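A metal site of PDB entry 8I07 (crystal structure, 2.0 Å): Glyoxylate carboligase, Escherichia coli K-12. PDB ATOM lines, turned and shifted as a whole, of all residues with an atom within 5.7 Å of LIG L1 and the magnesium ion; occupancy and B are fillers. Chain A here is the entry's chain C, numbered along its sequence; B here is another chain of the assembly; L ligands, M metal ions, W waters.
N of Asp 447 lies close to O3 of LIG L1. N of Leu 396 is in hydrogen-bond range of O7 of LIG L1. The backbone NH (N) of Gly 478 lies within hydrogen-bond range of an oxygen (O7) of LIG L1, at 3.4 Å. A nitrogen (N3) of LIG L1 is in hydrogen-bond range of the backbone carbonyl oxygen (O) of Gly 420, 2.8 Å away. An oxygen (O3) of LIG L1 sits close to the backbone NH (N) of Phe 448, 2.9 Å away. N of Asp 449 sits at hydrogen-bond distance from O2 of LIG L1 (2.9 Å). N of Leu 479 sits at hydrogen-bond distance from O7 of LIG L1 (2.9 Å). N of Ser 397 sits at hydrogen-bond distance from O6 of LIG L1 (3.0 Å). The side-chain amide nitrogen of Gln 116 of chain B sits close to a nitrogen (N3) of LIG L1 (3.2 Å). O2 of LG2 L2 is in hydrogen-bond range of N of Ala 29 of chain B (3.1 Å).
The magnesium ion is bound by an oxygen (O5) of LIG L1 (2.1 Å). O3 of LIG L1 binds the magnesium ion, 2.1 Å away. The magnesium ion is bound by OD1 of Asn 474 (2.1 Å). The backbone carbonyl oxygen (O) of Tyr 476 is bound to the magnesium ion (2.2 Å). The magnesium ion is bound by OD1 of Asp 447. Water W3 is bound to the magnesium ion (2.2 Å). The magnesium ion has six donor atoms within binding distance.
The side-chain carboxylate (OD2) of Asp 447 sits close to the backbone NH (N) of Ala 475. The side-chain carboxylate (OD2) of Asp 447 sits close to the side-chain amide oxygen (OD1) of Asn 473, 3.3 Å away. The backbone carbonyl oxygen of Gly 420 is in hydrogen-bond range of the side-chain amide nitrogen of Gln 116 of chain B (3.2 Å). The side-chain carboxylate (OD2) of Asp 449 is in hydrogen-bond range of the side-chain hydroxyl (OG) of Ser 445. The backbone NH of Gly 446 sits at hydrogen-bond distance from the side-chain hydroxyl of Ser 397 (3.2 Å). NE2 of Gln 116 of chain B sits at hydrogen-bond distance from O of Ala 419.
Water W3 lies within hydrogen-bond range of O6 of LIG L1, O of Val 472 and ND2 of Asn 474. Water W2 lies within hydrogen-bond range of O of Ile 394 (2.7 Å), N of Gly 446 (2.7 Å), OG of Ser 397 (2.7 Å) and O2 of LIG L1 (2.7 Å). Water W4 lies within hydrogen-bond range of O of Val 26 of chain B (2.7 Å), N of Thr 76 of chain B (2.8 Å) and N1 of LIG L1 (3.2 Å).
N of Gly 478 touches the magnesium ion (3.9 Å). Of the 36 residues printed, 4 come within 4 Å of the magnesium ion. The nearest printed residue that does not touch the magnesium ion is Leu 477 (4.3 Å).
Ile 394 touches LIG L1. Gly 395 touches LIG L1. N of Leu 422 touches N2 of LIG L1 (3.6 Å). Gly 446 touches LIG L1. Phe 452 touches LIG L1. Leu 477 touches LIG L1. CG1 of Ile 480 touches C9 of LIG L1, 3.5 Å away. CG1 of Val 26 of chain B touches C10 of LIG L1, at 3.96 Å. Pro 27 of chain B touches LIG L1 (O to C10, 3.4 Å). Val 52 of chain B touches LIG L1. Thr 76 of chain B touches LIG L1 (CG2 to C5, 3.6 Å). Pro 79 of chain B touches LIG L1. Ala 80 of chain B touches LIG L1. Asp 83 of chain B touches LIG L1. Within 4 Å of LIG L1: Ile 394, Gly 395, Leu 396, Ser 397, Gly 420, Leu 422, Gly 446, Asp 447, Phe 448, Asp 449, Phe 452, Asn 474, Tyr 476, Leu 477, Gly 478, Leu 479, Ile 480, Val 26 of chain B, Pro 27 of chain B, Val 52 of chain B, Thr 76 of chain B, Pro 79 of chain B, Ala 80 of chain B, Asp 83 of chain B and Gln 116 of chain B. Along chain A the residues within 4 Å of LIG L1 span positions 394 to 480. The nearest printed residue that does not touch LIG L1 is Pro 421 (4.2 Å).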
ATOM      1  N   ILE A 394       1.402   0.144   8.143  1.00  0.00           N
ATOM      2  CA  ILE A 394       0.990   0.299   9.536  1.00  0.00           C
ATOM      3  C   ILE A 394      -0.109  -0.708   9.864  1.00  0.00           C
ATOM      4  O   ILE A 394      -0.817  -1.192   8.973  1.00  0.00           O
ATOM      5  CB  ILE A 394       0.514   1.748   9.831  1.00  0.00           C
ATOM      6  CG1 ILE A 394       0.579   2.022  11.335  1.00  0.00           C
ATOM      7  CG2 ILE A 394      -0.906   1.958   9.345  1.00  0.00           C
ATOM      8  CD1 ILE A 394       0.191   3.423  11.730  1.00  0.00           C
ATOM      9  N   GLY A 395      -0.282  -0.982  11.141  1.00  0.00           N
ATOM     10  CA  GLY A 395      -1.225  -1.971  11.625  1.00  0.00           C
ATOM     11  C   GLY A 395      -0.524  -3.025  12.449  1.00  0.00           C
ATOM     12  O   GLY A 395       0.706  -3.082  12.536  1.00  0.00           O
ATOM     13  N   LEU A 396      -1.343  -3.879  13.081  1.00  0.00           N
ATOM     14  CA  LEU A 396      -0.758  -5.019  13.788  1.00  0.00           C
ATOM     15  C   LEU A 396       0.028  -5.896  12.823  1.00  0.00           C
ATOM     16  O   LEU A 396       1.038  -6.505  13.193  1.00  0.00           O
ATOM     17  CB  LEU A 396      -1.849  -5.815  14.507  1.00  0.00           C
ATOM     18  CG  LEU A 396      -2.614  -5.050  15.597  1.00  0.00           C
ATOM     19  CD1 LEU A 396      -3.595  -5.959  16.328  1.00  0.00           C
ATOM     20  CD2 LEU A 396      -1.655  -4.415  16.596  1.00  0.00           C
ATOM     21  N   SER A 397      -0.410  -5.942  11.565  1.00  0.00           N
ATOM     22  CA  SER A 397       0.323  -6.648  10.520  1.00  0.00           C
ATOM     23  C   SER A 397       1.750  -6.130  10.397  1.00  0.00           C
ATOM     24  O   SER A 397       2.701  -6.923  10.322  1.00  0.00           O
ATOM     25  CB  SER A 397      -0.415  -6.472   9.193  1.00  0.00           C
ATOM     26  OG  SER A 397      -0.735  -5.080   9.027  1.00  0.00           O
ATOM     27  N   GLN A 398       1.914  -4.794  10.366  1.00  0.00           N
ATOM     28  CA  GLN A 398       3.228  -4.180  10.192  1.00  0.00           C
ATOM     29  C   GLN A 398       4.047  -4.238  11.480  1.00  0.00           C
ATOM     30  O   GLN A 398       5.265  -4.464  11.430  1.00  0.00           O
ATOM     31  CB  GLN A 398       3.079  -2.719   9.739  1.00  0.00           C
ATOM     32  CG  GLN A 398       4.393  -1.937   9.694  1.00  0.00           C
ATOM     33  CD  GLN A 398       4.575  -0.972  10.890  1.00  0.00           C
ATOM     34  OE1 GLN A 398       3.702  -0.882  11.764  1.00  0.00           O
ATOM     35  NE2 GLN A 398       5.699  -0.256  10.913  1.00  0.00           N
ATOM     36  N   ALA A 419       4.689   8.721   9.107  1.00  0.00           N
ATOM     37  CA  ALA A 419       3.322   9.108   8.740  1.00  0.00           C
ATOM     38  C   ALA A 419       2.356   7.943   8.626  1.00  0.00           C
ATOM     39  O   ALA A 419       1.177   8.097   8.971  1.00  0.00           O
ATOM     40  CB  ALA A 419       3.324   9.887   7.424  1.00  0.00           C
ATOM     41  N   GLY A 420       2.781   6.796   8.116  1.00  0.00           N
ATOM     42  CA  GLY A 420       1.940   5.619   8.098  1.00  0.00           C
ATOM     43  C   GLY A 420       0.558   5.774   7.477  1.00  0.00           C
ATOM     44  O   GLY A 420      -0.446   5.367   8.071  1.00  0.00           O
ATOM     45  N   PRO A 421       0.468   6.376   6.290  1.00  0.00           N
ATOM     46  CA  PRO A 421      -0.839   6.498   5.623  1.00  0.00           C
ATOM     47  C   PRO A 421      -1.328   5.158   5.091  1.00  0.00           C
ATOM     48  O   PRO A 421      -0.620   4.492   4.328  1.00  0.00           O
ATOM     49  CB  PRO A 421      -0.549   7.467   4.468  1.00  0.00           C
ATOM     50  CG  PRO A 421       0.880   7.239   4.157  1.00  0.00           C
ATOM     51  CD  PRO A 421       1.560   6.963   5.492  1.00  0.00           C
ATOM     52  N   LEU A 422      -2.555   4.786   5.435  1.00  0.00           N
ATOM     53  CA  LEU A 422      -3.126   3.550   4.913  1.00  0.00           C
ATOM     54  C   LEU A 422      -3.281   3.641   3.400  1.00  0.00           C
ATOM     55  O   LEU A 422      -3.526   4.715   2.841  1.00  0.00           O
ATOM     56  CB  LEU A 422      -4.480   3.237   5.565  1.00  0.00           C
ATOM     57  CG  LEU A 422      -4.400   2.812   7.033  1.00  0.00           C
ATOM     58  CD1 LEU A 422      -5.759   2.917   7.732  1.00  0.00           C
ATOM     59  CD2 LEU A 422      -3.832   1.385   7.183  1.00  0.00           C
ATOM     60  N   SER A 445       0.411  -6.376   4.257  1.00  0.00           N
ATOM     61  CA  SER A 445      -0.693  -5.498   4.613  1.00  0.00           C
ATOM     62  C   SER A 445      -1.708  -6.238   5.460  1.00  0.00           C
ATOM     63  O   SER A 445      -1.929  -7.444   5.281  1.00  0.00           O
ATOM     64  CB  SER A 445      -1.441  -4.974   3.382  1.00  0.00           C
ATOM     65  OG  SER A 445      -0.585  -4.237   2.544  1.00  0.00           O
ATOM     66  N   GLY A 446      -2.357  -5.487   6.354  1.00  0.00           N
ATOM     67  CA  GLY A 446      -3.644  -5.905   6.876  1.00  0.00           C
ATOM     68  C   GLY A 446      -4.755  -5.660   5.871  1.00  0.00           C
ATOM     69  O   GLY A 446      -4.549  -5.046   4.833  1.00  0.00           O
ATOM     70  N   ASP A 447      -5.956  -6.181   6.190  1.00  0.00           N
ATOM     71  CA  ASP A 447      -7.070  -6.072   5.240  1.00  0.00           C
ATOM     72  C   ASP A 447      -7.495  -4.620   5.005  1.00  0.00           C
ATOM     73  O   ASP A 447      -7.822  -4.245   3.876  1.00  0.00           O
ATOM     74  CB  ASP A 447      -8.259  -6.932   5.690  1.00  0.00           C
ATOM     75  CG  ASP A 447      -8.640  -6.765   7.180  1.00  0.00           C
ATOM     76  OD1 ASP A 447      -7.753  -6.760   8.073  1.00  0.00           O
ATOM     77  OD2 ASP A 447      -9.858  -6.668   7.455  1.00  0.00           O
ATOM     78  N   PHE A 448      -7.463  -3.785   6.041  1.00  0.00           N
ATOM     79  CA  PHE A 448      -7.926  -2.402   5.889  1.00  0.00           C
ATOM     80  C   PHE A 448      -6.944  -1.583   5.051  1.00  0.00           C
ATOM     81  O   PHE A 448      -7.338  -0.898   4.096  1.00  0.00           O
ATOM     82  CB  PHE A 448      -8.131  -1.780   7.269  1.00  0.00           C
ATOM     83  CG  PHE A 448      -9.011  -0.546   7.289  1.00  0.00           C
ATOM     84  CD1 PHE A 448     -10.275  -0.556   6.711  1.00  0.00           C
ATOM     85  CD2 PHE A 448      -8.595   0.607   7.942  1.00  0.00           C
ATOM     86  CE1 PHE A 448     -11.086   0.578   6.749  1.00  0.00           C
ATOM     87  CE2 PHE A 448      -9.404   1.716   8.002  1.00  0.00           C
ATOM     88  CZ  PHE A 448     -10.647   1.708   7.396  1.00  0.00           C
ATOM     89  N   ASP A 449      -5.645  -1.670   5.365  1.00  0.00           N
ATOM     90  CA  ASP A 449      -4.643  -1.030   4.523  1.00  0.00           C
ATOM     91  C   ASP A 449      -4.766  -1.502   3.085  1.00  0.00           C
ATOM     92  O   ASP A 449      -4.722  -0.693   2.152  1.00  0.00           O
ATOM     93  CB  ASP A 449      -3.229  -1.326   5.064  1.00  0.00           C
ATOM     94  CG  ASP A 449      -2.121  -1.025   4.047  1.00  0.00           C
ATOM     95  OD1 ASP A 449      -2.100   0.086   3.475  1.00  0.00           O
ATOM     96  OD2 ASP A 449      -1.257  -1.897   3.850  1.00  0.00           O
ATOM     97  N   PHE A 450      -4.975  -2.810   2.893  1.00  0.00           N
ATOM     98  CA  PHE A 450      -5.080  -3.370   1.557  1.00  0.00           C
ATOM     99  C   PHE A 450      -6.239  -2.763   0.789  1.00  0.00           C
ATOM    100  O   PHE A 450      -6.160  -2.584  -0.436  1.00  0.00           O
ATOM    101  CB  PHE A 450      -5.241  -4.889   1.688  1.00  0.00           C
ATOM    102  CG  PHE A 450      -5.068  -5.653   0.390  1.00  0.00           C
ATOM    103  CD1 PHE A 450      -3.824  -5.793  -0.180  1.00  0.00           C
ATOM    104  CD2 PHE A 450      -6.154  -6.286  -0.202  1.00  0.00           C
ATOM    105  CE1 PHE A 450      -3.675  -6.509  -1.360  1.00  0.00           C
ATOM    106  CE2 PHE A 450      -6.009  -7.014  -1.364  1.00  0.00           C
ATOM    107  CZ  PHE A 450      -4.773  -7.118  -1.939  1.00  0.00           C
ATOM    108  N   PHE A 452      -7.689   0.349   1.046  1.00  0.00           N
ATOM    109  CA  PHE A 452      -7.730   1.792   0.770  1.00  0.00           C
ATOM    110  C   PHE A 452      -7.484   2.088  -0.697  1.00  0.00           C
ATOM    111  O   PHE A 452      -8.251   2.822  -1.339  1.00  0.00           O
ATOM    112  CB  PHE A 452      -6.674   2.529   1.595  1.00  0.00           C
ATOM    113  CG  PHE A 452      -7.183   3.196   2.853  1.00  0.00           C
ATOM    114  CD1 PHE A 452      -7.898   2.481   3.808  1.00  0.00           C
ATOM    115  CD2 PHE A 452      -6.878   4.521   3.105  1.00  0.00           C
ATOM    116  CE1 PHE A 452      -8.327   3.101   4.979  1.00  0.00           C
ATOM    117  CE2 PHE A 452      -7.313   5.153   4.271  1.00  0.00           C
ATOM    118  CZ  PHE A 452      -8.029   4.438   5.204  1.00  0.00           C
ATOM    119  N   VAL A 472      -2.745 -10.279   5.541  1.00  0.00           N
ATOM    120  CA  VAL A 472      -3.173 -10.917   6.787  1.00  0.00           C
ATOM    121  C   VAL A 472      -4.509 -10.298   7.174  1.00  0.00           C
ATOM    122  O   VAL A 472      -4.595  -9.128   7.567  1.00  0.00           O
ATOM    123  CB  VAL A 472      -2.110 -10.764   7.898  1.00  0.00           C
ATOM    124  CG1 VAL A 472      -0.824 -11.519   7.500  1.00  0.00           C
ATOM    125  CG2 VAL A 472      -1.805  -9.295   8.189  1.00  0.00           C
ATOM    126  N   ASN A 473      -5.584 -11.088   7.038  1.00  0.00           N
ATOM    127  CA  ASN A 473      -6.955 -10.609   7.104  1.00  0.00           C
ATOM    128  C   ASN A 473      -7.601 -11.042   8.409  1.00  0.00           C
ATOM    129  O   ASN A 473      -7.852 -12.233   8.616  1.00  0.00           O
ATOM    130  CB  ASN A 473      -7.761 -11.140   5.918  1.00  0.00           C
ATOM    131  CG  ASN A 473      -9.206 -10.714   5.959  1.00  0.00           C
ATOM    132  OD1 ASN A 473      -9.618  -9.937   6.834  1.00  0.00           O
ATOM    133  ND2 ASN A 473      -9.997 -11.197   5.013  1.00  0.00           N
ATOM    134  N   ASN A 474      -7.895 -10.086   9.283  1.00  0.00           N
ATOM    135  CA  ASN A 474      -8.644 -10.361  10.505  1.00  0.00           C
ATOM    136  C   ASN A 474     -10.026  -9.723  10.485  1.00  0.00           C
ATOM    137  O   ASN A 474     -10.725  -9.752  11.507  1.00  0.00           O
ATOM    138  CB  ASN A 474      -7.856  -9.877  11.733  1.00  0.00           C
ATOM    139  CG  ASN A 474      -7.379  -8.451  11.599  1.00  0.00           C
ATOM    140  OD1 ASN A 474      -7.882  -7.685  10.776  1.00  0.00           O
ATOM    141  ND2 ASN A 474      -6.393  -8.076  12.410  1.00  0.00           N
ATOM    142  N   ALA A 475     -10.448  -9.160   9.361  1.00  0.00           N
ATOM    143  CA  ALA A 475     -11.717  -8.443   9.267  1.00  0.00           C
ATOM    144  C   ALA A 475     -11.850  -7.393  10.373  1.00  0.00           C
ATOM    145  O   ALA A 475     -12.915  -7.203  10.960  1.00  0.00           O
ATOM    146  CB  ALA A 475     -12.901  -9.418   9.283  1.00  0.00           C
ATOM    147  N   TYR A 476     -10.739  -6.702  10.647  1.00  0.00           N
ATOM    148  CA  TYR A 476     -10.624  -5.764  11.761  1.00  0.00           C
ATOM    149  C   TYR A 476      -9.662  -4.638  11.409  1.00  0.00           C
ATOM    150  O   TYR A 476      -8.702  -4.834  10.668  1.00  0.00           O
ATOM    151  CB  TYR A 476     -10.072  -6.450  13.020  1.00  0.00           C
ATOM    152  CG  TYR A 476     -11.032  -6.699  14.176  1.00  0.00           C
ATOM    153  CD1 TYR A 476     -11.421  -5.679  15.026  1.00  0.00           C
ATOM    154  CD2 TYR A 476     -11.478  -7.991  14.460  1.00  0.00           C
ATOM    155  CE1 TYR A 476     -12.266  -5.914  16.088  1.00  0.00           C
ATOM    156  CE2 TYR A 476     -12.312  -8.245  15.523  1.00  0.00           C
ATOM    157  CZ  TYR A 476     -12.710  -7.209  16.337  1.00  0.00           C
ATOM    158  OH  TYR A 476     -13.540  -7.451  17.404  1.00  0.00           O
ATOM    159  N   LEU A 477      -9.906  -3.462  11.994  1.00  0.00           N
ATOM    160  CA  LEU A 477      -8.815  -2.494  12.191  1.00  0.00           C
ATOM    161  C   LEU A 477      -8.119  -2.924  13.476  1.00  0.00           C
ATOM    162  O   LEU A 477      -8.353  -2.409  14.571  1.00  0.00           O
ATOM    163  CB  LEU A 477      -9.310  -1.063  12.280  1.00  0.00           C
ATOM    164  CG  LEU A 477     -10.516  -0.515  11.523  1.00  0.00           C
ATOM    165  CD1 LEU A 477     -10.487   1.042  11.512  1.00  0.00           C
ATOM    166  CD2 LEU A 477     -10.742  -1.107  10.128  1.00  0.00           C
ATOM    167  N   GLY A 478      -7.245  -3.929  13.342  1.00  0.00           N
ATOM    168  CA  GLY A 478      -6.773  -4.639  14.524  1.00  0.00           C
ATOM    169  C   GLY A 478      -5.965  -3.761  15.467  1.00  0.00           C
ATOM    170  O   GLY A 478      -6.126  -3.837  16.680  1.00  0.00           O
ATOM    171  N   LEU A 479      -5.130  -2.889  14.906  1.00  0.00           N
ATOM    172  CA  LEU A 479      -4.361  -2.006  15.783  1.00  0.00           C
ATOM    173  C   LEU A 479      -5.291  -1.069  16.554  1.00  0.00           C
ATOM    174  O   LEU A 479      -5.037  -0.762  17.717  1.00  0.00           O
ATOM    175  CB  LEU A 479      -3.337  -1.221  14.953  1.00  0.00           C
ATOM    176  CG  LEU A 479      -2.499  -0.159  15.697  1.00  0.00           C
ATOM    177  CD1 LEU A 479      -1.838  -0.733  16.953  1.00  0.00           C
ATOM    178  CD2 LEU A 479      -1.447   0.468  14.769  1.00  0.00           C
ATOM    179  N   ILE A 480      -6.394  -0.633  15.933  1.00  0.00           N
ATOM    180  CA  ILE A 480      -7.279   0.320  16.587  1.00  0.00           C
ATOM    181  C   ILE A 480      -8.134  -0.388  17.639  1.00  0.00           C
ATOM    182  O   ILE A 480      -8.421   0.180  18.704  1.00  0.00           O
ATOM    183  CB  ILE A 480      -8.145   1.084  15.559  1.00  0.00           C
ATOM    184  CG1 ILE A 480      -7.258   1.671  14.457  1.00  0.00           C
ATOM    185  CG2 ILE A 480      -8.899   2.233  16.216  1.00  0.00           C
ATOM    186  CD1 ILE A 480      -6.120   2.493  14.993  1.00  0.00           C
ATOM    187  N   LEU A 495     -14.815  -4.997  10.220  1.00  0.00           N
ATOM    188  CA  LEU A 495     -15.091  -4.955   8.787  1.00  0.00           C
ATOM    189  C   LEU A 495     -15.881  -6.166   8.302  1.00  0.00           C
ATOM    190  O   LEU A 495     -16.195  -6.245   7.108  1.00  0.00           O
ATOM    191  CB  LEU A 495     -13.786  -4.848   8.003  1.00  0.00           C
ATOM    192  CG  LEU A 495     -12.863  -3.674   8.368  1.00  0.00           C
ATOM    193  CD1 LEU A 495     -11.483  -3.855   7.732  1.00  0.00           C
ATOM    194  CD2 LEU A 495     -13.500  -2.366   7.939  1.00  0.00           C
ATOM    195  N   VAL B  26     -13.132   7.075  10.088  1.00  0.00           N
ATOM    196  CA  VAL B  26     -12.170   6.013  10.310  1.00  0.00           C
ATOM    197  C   VAL B  26     -11.527   6.292  11.668  1.00  0.00           C
ATOM    198  O   VAL B  26     -10.842   7.324  11.813  1.00  0.00           O
ATOM    199  CB  VAL B  26     -11.123   5.968   9.194  1.00  0.00           C
ATOM    200  CG1 VAL B  26     -10.069   4.870   9.476  1.00  0.00           C
ATOM    201  CG2 VAL B  26     -11.792   5.757   7.849  1.00  0.00           C
ATOM    202  N   PRO B  27     -11.738   5.460  12.682  1.00  0.00           N
ATOM    203  CA  PRO B  27     -11.107   5.676  13.983  1.00  0.00           C
ATOM    204  C   PRO B  27      -9.601   5.447  13.943  1.00  0.00           C
ATOM    205  O   PRO B  27      -9.064   4.752  13.069  1.00  0.00           O
ATOM    206  CB  PRO B  27     -11.803   4.659  14.881  1.00  0.00           C
ATOM    207  CG  PRO B  27     -12.172   3.551  13.954  1.00  0.00           C
ATOM    208  CD  PRO B  27     -12.544   4.220  12.649  1.00  0.00           C
ATOM    209  N   GLY B  28      -8.914   6.073  14.899  1.00  0.00           N
ATOM    210  CA  GLY B  28      -7.505   5.828  15.126  1.00  0.00           C
ATOM    211  C   GLY B  28      -7.193   6.170  16.569  1.00  0.00           C
ATOM    212  O   GLY B  28      -8.055   6.679  17.306  1.00  0.00           O
ATOM    213  N   ALA B  29      -5.948   5.919  16.962  1.00  0.00           N
ATOM    214  CA  ALA B  29      -5.602   6.055  18.374  1.00  0.00           C
ATOM    215  C   ALA B  29      -5.817   7.481  18.867  1.00  0.00           C
ATOM    216  O   ALA B  29      -6.328   7.695  19.976  1.00  0.00           O
ATOM    217  CB  ALA B  29      -4.157   5.605  18.614  1.00  0.00           C
ATOM    218  N   VAL B  52     -10.155   7.171   4.158  1.00  0.00           N
ATOM    219  CA  VAL B  52     -10.556   8.407   4.823  1.00  0.00           C
ATOM    220  C   VAL B  52     -11.121   9.392   3.808  1.00  0.00           C
ATOM    221  O   VAL B  52     -12.052  10.142   4.106  1.00  0.00           O
ATOM    222  CB  VAL B  52      -9.397   9.023   5.624  1.00  0.00           C
ATOM    223  CG1 VAL B  52      -9.723  10.474   5.946  1.00  0.00           C
ATOM    224  CG2 VAL B  52      -9.188   8.235   6.912  1.00  0.00           C
ATOM    225  N   THR B  76      -8.305  10.172  12.467  1.00  0.00           N
ATOM    226  CA  THR B  76      -7.245  10.262  13.462  1.00  0.00           C
ATOM    227  C   THR B  76      -6.271  11.385  13.084  1.00  0.00           C
ATOM    228  O   THR B  76      -6.625  12.296  12.305  1.00  0.00           O
ATOM    229  CB  THR B  76      -6.546   8.910  13.608  1.00  0.00           C
ATOM    230  OG1 THR B  76      -5.768   8.880  14.808  1.00  0.00           O
ATOM    231  CG2 THR B  76      -5.657   8.590  12.396  1.00  0.00           C
ATOM    232  N   PRO B  79      -1.903  11.404   8.726  1.00  0.00           N
ATOM    233  CA  PRO B  79      -2.381  11.219   7.340  1.00  0.00           C
ATOM    234  C   PRO B  79      -3.899  11.314   7.180  1.00  0.00           C
ATOM    235  O   PRO B  79      -4.370  11.557   6.055  1.00  0.00           O
ATOM    236  CB  PRO B  79      -1.849   9.828   6.977  1.00  0.00           C
ATOM    237  CG  PRO B  79      -1.823   9.101   8.296  1.00  0.00           C
ATOM    238  CD  PRO B  79      -1.374  10.152   9.288  1.00  0.00           C
ATOM    239  N   ALA B  80      -4.681  11.027   8.215  1.00  0.00           N
ATOM    240  CA  ALA B  80      -6.127  11.138   8.053  1.00  0.00           C
ATOM    241  C   ALA B  80      -6.539  12.562   7.724  1.00  0.00           C
ATOM    242  O   ALA B  80      -7.383  12.787   6.851  1.00  0.00           O
ATOM    243  CB  ALA B  80      -6.850  10.636   9.315  1.00  0.00           C
ATOM    244  N   ASP B  83      -5.682  13.329   4.147  1.00  0.00           N
ATOM    245  CA  ASP B  83      -6.629  12.639   3.279  1.00  0.00           C
ATOM    246  C   ASP B  83      -7.962  13.367   3.172  1.00  0.00           C
ATOM    247  O   ASP B  83      -8.792  12.979   2.334  1.00  0.00           O
ATOM    248  CB  ASP B  83      -6.878  11.215   3.778  1.00  0.00           C
ATOM    249  CG  ASP B  83      -5.831  10.208   3.303  1.00  0.00           C
ATOM    250  OD1 ASP B  83      -4.955  10.566   2.499  1.00  0.00           O
ATOM    251  OD2 ASP B  83      -5.912   9.034   3.752  1.00  0.00           O
ATOM    252  N   GLN B 116       2.860  10.421  13.643  1.00  0.00           N
ATOM    253  CA  GLN B 116       1.637  10.779  12.932  1.00  0.00           C
ATOM    254  C   GLN B 116       1.057  12.117  13.409  1.00  0.00           C
ATOM    255  O   GLN B 116      -0.152  12.255  13.598  1.00  0.00           O
ATOM    256  CB  GLN B 116       0.594   9.661  13.062  1.00  0.00           C
ATOM    257  CG  GLN B 116       0.933   8.406  12.260  1.00  0.00           C
ATOM    258  CD  GLN B 116      -0.270   7.494  12.062  1.00  0.00           C
ATOM    259  OE1 GLN B 116      -1.027   7.217  12.992  1.00  0.00           O
ATOM    260  NE2 GLN B 116      -0.450   7.013  10.826  1.00  0.00           N
HETATM  261  N1  LIG L   1      -6.408   6.690   8.796  1.00  0.00           N
HETATM  262  C1  LIG L   1      -5.328   6.768   8.005  1.00  0.00           C
HETATM  263  C2  LIG L   1      -5.489   7.469   6.689  1.00  0.00           C
HETATM  264  N2  LIG L   1      -4.117   6.267   8.288  1.00  0.00           N
HETATM  265  C3  LIG L   1      -3.962   5.630   9.464  1.00  0.00           C
HETATM  266  N3  LIG L   1      -2.744   5.134   9.724  1.00  0.00           N
HETATM  267  C4  LIG L   1      -5.059   5.465  10.368  1.00  0.00           C
HETATM  268  C5  LIG L   1      -6.244   6.037   9.963  1.00  0.00           C
HETATM  269  C6  LIG L   1      -4.949   4.796  11.711  1.00  0.00           C
HETATM  270  N4  LIG L   1      -4.679   3.336  11.659  1.00  0.00           N
HETATM  271  C7  LIG L   1      -3.496   2.804  11.948  1.00  0.00           C
HETATM  272  S1  LIG L   1      -3.495   1.127  11.842  1.00  0.00           S
HETATM  273  C8  LIG L   1      -5.182   1.123  11.450  1.00  0.00           C
HETATM  274  C9  LIG L   1      -5.673   2.398  11.393  1.00  0.00           C
HETATM  275  C10 LIG L   1      -7.064   2.828  11.062  1.00  0.00           C
HETATM  276  C11 LIG L   1      -5.895  -0.174  11.165  1.00  0.00           C
HETATM  277  C12 LIG L   1      -5.114  -1.060  10.232  1.00  0.00           C
HETATM  278  O1  LIG L   1      -5.903  -2.242   9.939  1.00  0.00           O
HETATM  279  P1  LIG L   1      -5.417  -3.398   9.016  1.00  0.00           P
HETATM  280  O2  LIG L   1      -4.642  -2.718   7.872  1.00  0.00           O
HETATM  281  O3  LIG L   1      -6.478  -4.367   8.676  1.00  0.00           O
HETATM  282  O4  LIG L   1      -4.375  -4.051   9.998  1.00  0.00           O
HETATM  283  P2  LIG L   1      -4.400  -4.889  11.351  1.00  0.00           P
HETATM  284  O5  LIG L   1      -5.789  -5.387  11.585  1.00  0.00           O
HETATM  285  O6  LIG L   1      -3.384  -6.008  11.128  1.00  0.00           O
HETATM  286  O7  LIG L   1      -3.964  -3.893  12.424  1.00  0.00           O
HETATM  287  C1  LG2 L   2      -1.693   4.433  16.388  1.00  0.00           C
HETATM  288  C2  LG2 L   2      -2.451   4.218  15.077  1.00  0.00           C
HETATM  289  O1  LG2 L   2      -0.714   3.812  16.638  1.00  0.00           O
HETATM  290  O2  LG2 L   2      -3.729   4.779  15.176  1.00  0.00           O
HETATM  291 MG    MG M   1      -6.992  -5.948   9.966  1.00  0.00          MG
HETATM  292  O   HOH W   1      -2.749  -8.574  11.959  1.00  0.00           O
HETATM  293  O   HOH W   2      -2.013  -3.175   7.650  1.00  0.00           O
HETATM  294  O   HOH W   3      -5.228  -7.265   9.577  1.00  0.00           O
HETATM  295  O   HOH W   4      -8.650   8.172  10.499  1.00  0.00           O
